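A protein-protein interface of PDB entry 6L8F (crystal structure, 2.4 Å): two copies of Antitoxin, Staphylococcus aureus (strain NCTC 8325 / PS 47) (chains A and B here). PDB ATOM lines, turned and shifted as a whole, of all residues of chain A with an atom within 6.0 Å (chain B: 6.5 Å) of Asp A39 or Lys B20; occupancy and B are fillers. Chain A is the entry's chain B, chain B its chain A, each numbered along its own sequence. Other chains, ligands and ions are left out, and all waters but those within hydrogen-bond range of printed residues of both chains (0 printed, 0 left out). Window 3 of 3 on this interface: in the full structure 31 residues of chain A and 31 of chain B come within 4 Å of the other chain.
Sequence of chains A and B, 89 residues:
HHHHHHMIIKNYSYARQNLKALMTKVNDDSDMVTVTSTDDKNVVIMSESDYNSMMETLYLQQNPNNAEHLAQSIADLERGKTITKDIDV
The side-chain hydroxyl of Tyr A12 lies within hydrogen-bond range of the backbone NH of Lys B20, 2.9 Å away.
OD2 of Asp A39 lies close to NZ of Lys B20 (2.4 Å).
OG of Ser A37 sits at hydrogen-bond distance from N of Lys A41 (3.2 Å).
O of Lys B20 is in hydrogen-bond range of OG1 of Thr B24 (2.7 Å).
N of Asp A39 sits close to OG of Ser A37.
Tyr A12 touches Leu B19.
CB of Ser A37 touches CE of Lys B20 (3.8 Å).
Ser A37 touches Met B23 (CB to CE, 3.9 Å).
Lys A41 touches Met B23 (O to CE, 3.6 Å).
Of chain B, only Lys B20 (2.4 Å) comes within 4 Å of Asp A39.
Of chain A, only Tyr A12 (2.9 Å), Ser A37 (3.8 Å) and Asp A39 (2.4 Å) come within 4 Å of Lys B20.
Of the printed residues of chain B, Lys A41 touches Met B23.
Of the printed residues of chain A, Leu B19 touches Tyr A12 (3.5 Å).
Printed residues of chain A within 4 Å of Met B23: Ser A37 (3.9 Å) and Lys A41 (3.6 Å).
Leu B22 touches none of the printed residues of chain A.
The nearest residue of chain B that does not touch Asp A39 is Thr B24 (5.5 Å).
The nearest printed residue of chain A that does not touch Leu B19 is Lys A41 (8.2 Å).
Of the 10 printed residues of chain B, 3 touch a printed residue of chain A.
Hydrophobic or aromatic side chains of chain B that line the printed part of chain A: Leu B19 and Met B23.
Printed residues of chain A that touch a printed residue of chain B: Tyr A12, Ser A37, Asp A39 and Lys A41.
Among the printed residues, Asp or Glu carboxylates within 4 Å of a Lys or Arg side-chain nitrogen of the other chain: Asp A39 with Lys B20 (2.4 Å).
No position is printed for both chains.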
ATOM      1  N   TYR A  12      12.886 -20.567  14.644  1.00  0.00           N
ATOM      2  CA  TYR A  12      12.110 -21.174  13.564  1.00  0.00           C
ATOM      3  C   TYR A  12      11.992 -22.676  13.775  1.00  0.00           C
ATOM      4  O   TYR A  12      10.878 -23.186  13.922  1.00  0.00           O
ATOM      5  CB  TYR A  12      12.746 -20.890  12.187  1.00  0.00           C
ATOM      6  CG  TYR A  12      11.942 -21.264  10.910  1.00  0.00           C
ATOM      7  CD1 TYR A  12      11.741 -20.324   9.916  1.00  0.00           C
ATOM      8  CD2 TYR A  12      11.458 -22.566  10.665  1.00  0.00           C
ATOM      9  CE1 TYR A  12      11.045 -20.650   8.769  1.00  0.00           C
ATOM     10  CE2 TYR A  12      10.758 -22.888   9.538  1.00  0.00           C
ATOM     11  CZ  TYR A  12      10.558 -21.936   8.585  1.00  0.00           C
ATOM     12  OH  TYR A  12       9.863 -22.291   7.452  1.00  0.00           O
ATOM     13  N   SER A  37      14.162 -15.755  13.083  1.00  0.00           N
ATOM     14  CA  SER A  37      14.754 -16.293  11.869  1.00  0.00           C
ATOM     15  C   SER A  37      16.171 -15.758  11.719  1.00  0.00           C
ATOM     16  O   SER A  37      16.561 -14.780  12.365  1.00  0.00           O
ATOM     17  CB  SER A  37      13.926 -15.926  10.630  1.00  0.00           C
ATOM     18  OG  SER A  37      13.965 -14.527  10.392  1.00  0.00           O
ATOM     19  N   THR A  38      16.944 -16.417  10.852  1.00  0.00           N
ATOM     20  CA  THR A  38      18.272 -15.931  10.493  1.00  0.00           C
ATOM     21  C   THR A  38      18.226 -14.797   9.474  1.00  0.00           C
ATOM     22  O   THR A  38      19.254 -14.154   9.238  1.00  0.00           O
ATOM     23  CB  THR A  38      19.131 -17.078   9.944  1.00  0.00           C
ATOM     24  OG1 THR A  38      18.467 -17.684   8.828  1.00  0.00           O
ATOM     25  CG2 THR A  38      19.372 -18.131  11.018  1.00  0.00           C
ATOM     26  N   ASP A  39      17.060 -14.536   8.882  1.00  0.00           N
ATOM     27  CA  ASP A  39      16.881 -13.492   7.883  1.00  0.00           C
ATOM     28  C   ASP A  39      16.582 -12.129   8.496  1.00  0.00           C
ATOM     29  O   ASP A  39      16.278 -11.191   7.747  1.00  0.00           O
ATOM     30  CB  ASP A  39      15.753 -13.880   6.922  1.00  0.00           C
ATOM     31  CG  ASP A  39      15.973 -15.241   6.286  1.00  0.00           C
ATOM     32  OD1 ASP A  39      17.071 -15.481   5.744  1.00  0.00           O
ATOM     33  OD2 ASP A  39      15.049 -16.078   6.339  1.00  0.00           O
ATOM     34  N   ASP A  40      16.664 -12.015   9.832  1.00  0.00           N
ATOM     35  CA  ASP A  40      16.310 -10.810  10.600  1.00  0.00           C
ATOM     36  C   ASP A  40      14.863 -10.383  10.334  1.00  0.00           C
ATOM     37  O   ASP A  40      14.537  -9.194  10.283  1.00  0.00           O
ATOM     38  CB  ASP A  40      17.291  -9.659  10.336  1.00  0.00           C
ATOM     39  CG  ASP A  40      17.329  -8.650  11.468  1.00  0.00           C
ATOM     40  OD1 ASP A  40      16.762  -8.943  12.544  1.00  0.00           O
ATOM     41  OD2 ASP A  40      17.917  -7.561  11.276  1.00  0.00           O
ATOM     42  N   LYS A  41      13.980 -11.366  10.162  1.00  0.00           N
ATOM     43  CA  LYS A  41      12.573 -11.119   9.873  1.00  0.00           C
ATOM     44  C   LYS A  41      11.734 -11.868  10.913  1.00  0.00           C
ATOM     45  O   LYS A  41      11.062 -12.859  10.613  1.00  0.00           O
ATOM     46  CB  LYS A  41      12.229 -11.531   8.439  1.00  0.00           C
ATOM     47  CG  LYS A  41      12.981 -10.725   7.381  1.00  0.00           C
ATOM     48  CD  LYS A  41      12.409 -10.928   5.983  1.00  0.00           C
ATOM     49  CE  LYS A  41      12.942  -9.880   5.004  1.00  0.00           C
ATOM     50  NZ  LYS A  41      14.275 -10.211   4.435  1.00  0.00           N
ATOM     51  N   ALA B  15      -0.248 -24.153   7.676  1.00  0.00           N
ATOM     52  CA  ALA B  15       0.747 -23.337   8.355  1.00  0.00           C
ATOM     53  C   ALA B  15       1.942 -24.134   8.865  1.00  0.00           C
ATOM     54  O   ALA B  15       2.950 -23.520   9.232  1.00  0.00           O
ATOM     55  CB  ALA B  15       0.092 -22.595   9.521  1.00  0.00           C
ATOM     56  N   GLN B  17       3.996 -26.509   7.238  1.00  0.00           N
ATOM     57  CA  GLN B  17       5.122 -26.603   6.325  1.00  0.00           C
ATOM     58  C   GLN B  17       5.258 -25.391   5.412  1.00  0.00           C
ATOM     59  O   GLN B  17       6.259 -25.287   4.695  1.00  0.00           O
ATOM     60  CB  GLN B  17       5.007 -27.894   5.503  1.00  0.00           C
ATOM     61  CG  GLN B  17       4.802 -29.129   6.387  1.00  0.00           C
ATOM     62  CD  GLN B  17       4.506 -30.389   5.598  1.00  0.00           C
ATOM     63  OE1 GLN B  17       4.776 -30.464   4.399  1.00  0.00           O
ATOM     64  NE2 GLN B  17       3.944 -31.388   6.270  1.00  0.00           N
ATOM     65  N   ASN B  18       4.296 -24.475   5.430  1.00  0.00           N
ATOM     66  CA  ASN B  18       4.444 -23.168   4.785  1.00  0.00           C
ATOM     67  C   ASN B  18       4.734 -22.081   5.813  1.00  0.00           C
ATOM     68  O   ASN B  18       4.063 -21.050   5.861  1.00  0.00           O
ATOM     69  CB  ASN B  18       3.198 -22.834   3.976  1.00  0.00           C
ATOM     70  CG  ASN B  18       3.140 -23.586   2.667  1.00  0.00           C
ATOM     71  OD1 ASN B  18       4.150 -23.728   1.974  1.00  0.00           O
ATOM     72  ND2 ASN B  18       1.954 -24.080   2.320  1.00  0.00           N
ATOM     73  N   LEU B  19       5.752 -22.299   6.652  1.00  0.00           N
ATOM     74  CA  LEU B  19       5.998 -21.377   7.754  1.00  0.00           C
ATOM     75  C   LEU B  19       6.820 -20.169   7.321  1.00  0.00           C
ATOM     76  O   LEU B  19       6.487 -19.037   7.688  1.00  0.00           O
ATOM     77  CB  LEU B  19       6.679 -22.094   8.918  1.00  0.00           C
ATOM     78  CG  LEU B  19       6.627 -21.285  10.217  1.00  0.00           C
ATOM     79  CD1 LEU B  19       5.186 -20.951  10.583  1.00  0.00           C
ATOM     80  CD2 LEU B  19       7.310 -22.025  11.355  1.00  0.00           C
ATOM     81  N   LYS B  20       7.894 -20.373   6.547  1.00  0.00           N
ATOM     82  CA  LYS B  20       8.645 -19.215   6.065  1.00  0.00           C
ATOM     83  C   LYS B  20       7.925 -18.520   4.925  1.00  0.00           C
ATOM     84  O   LYS B  20       8.163 -17.331   4.682  1.00  0.00           O
ATOM     85  CB  LYS B  20      10.052 -19.600   5.606  1.00  0.00           C
ATOM     86  CG  LYS B  20      11.097 -18.470   5.748  1.00  0.00           C
ATOM     87  CD  LYS B  20      10.830 -17.567   6.969  1.00  0.00           C
ATOM     88  CE  LYS B  20      12.088 -16.880   7.493  1.00  0.00           C
ATOM     89  NZ  LYS B  20      12.667 -15.879   6.548  1.00  0.00           N
ATOM     90  N   ALA B  21       7.055 -19.245   4.211  1.00  0.00           N
ATOM     91  CA  ALA B  21       6.266 -18.629   3.150  1.00  0.00           C
ATOM     92  C   ALA B  21       5.304 -17.595   3.710  1.00  0.00           C
ATOM     93  O   ALA B  21       5.000 -16.600   3.040  1.00  0.00           O
ATOM     94  CB  ALA B  21       5.504 -19.699   2.370  1.00  0.00           C
ATOM     95  N   LEU B  22       4.839 -17.799   4.942  1.00  0.00           N
ATOM     96  CA  LEU B  22       3.992 -16.828   5.618  1.00  0.00           C
ATOM     97  C   LEU B  22       4.802 -15.820   6.428  1.00  0.00           C
ATOM     98  O   LEU B  22       4.454 -14.636   6.437  1.00  0.00           O
ATOM     99  CB  LEU B  22       2.980 -17.556   6.511  1.00  0.00           C
ATOM    100  CG  LEU B  22       1.943 -18.379   5.736  1.00  0.00           C
ATOM    101  CD1 LEU B  22       1.144 -19.304   6.651  1.00  0.00           C
ATOM    102  CD2 LEU B  22       1.006 -17.473   4.937  1.00  0.00           C
ATOM    103  N   MET B  23       5.884 -16.263   7.085  1.00  0.00           N
ATOM    104  CA  MET B  23       6.704 -15.372   7.912  1.00  0.00           C
ATOM    105  C   MET B  23       7.352 -14.266   7.088  1.00  0.00           C
ATOM    106  O   MET B  23       7.467 -13.124   7.549  1.00  0.00           O
ATOM    107  CB  MET B  23       7.794 -16.163   8.637  1.00  0.00           C
ATOM    108  CG  MET B  23       7.394 -16.791   9.952  1.00  0.00           C
ATOM    109  SD  MET B  23       8.799 -17.636  10.720  1.00  0.00           S
ATOM    110  CE  MET B  23       9.999 -16.303  10.826  1.00  0.00           C
ATOM    111  N   THR B  24       7.787 -14.585   5.868  1.00  0.00           N
ATOM    112  CA  THR B  24       8.437 -13.575   5.042  1.00  0.00           C
ATOM    113  C   THR B  24       7.423 -12.575   4.496  1.00  0.00           C
ATOM    114  O   THR B  24       7.672 -11.365   4.522  1.00  0.00           O
ATOM    115  CB  THR B  24       9.215 -14.242   3.906  1.00  0.00           C
ATOM    116  OG1 THR B  24       9.949 -15.359   4.426  1.00  0.00           O
ATOM    117  CG2 THR B  24      10.193 -13.255   3.281  1.00  0.00           C
ATOM    118  N   LYS B  25       6.260 -13.055   4.035  1.00  0.00           N
ATOM    119  CA  LYS B  25       5.243 -12.151   3.506  1.00  0.00           C
ATOM    120  C   LYS B  25       4.568 -11.332   4.601  1.00  0.00           C
ATOM    121  O   LYS B  25       3.960 -10.299   4.300  1.00  0.00           O
ATOM    122  CB  LYS B  25       4.195 -12.932   2.708  1.00  0.00           C
ATOM    123  CG  LYS B  25       3.575 -12.112   1.575  1.00  0.00           C
ATOM    124  CD  LYS B  25       2.767 -12.952   0.591  1.00  0.00           C
ATOM    125  CE  LYS B  25       1.401 -13.296   1.142  1.00  0.00           C
ATOM    126  NZ  LYS B  25       0.540 -13.967   0.126  1.00  0.00           N
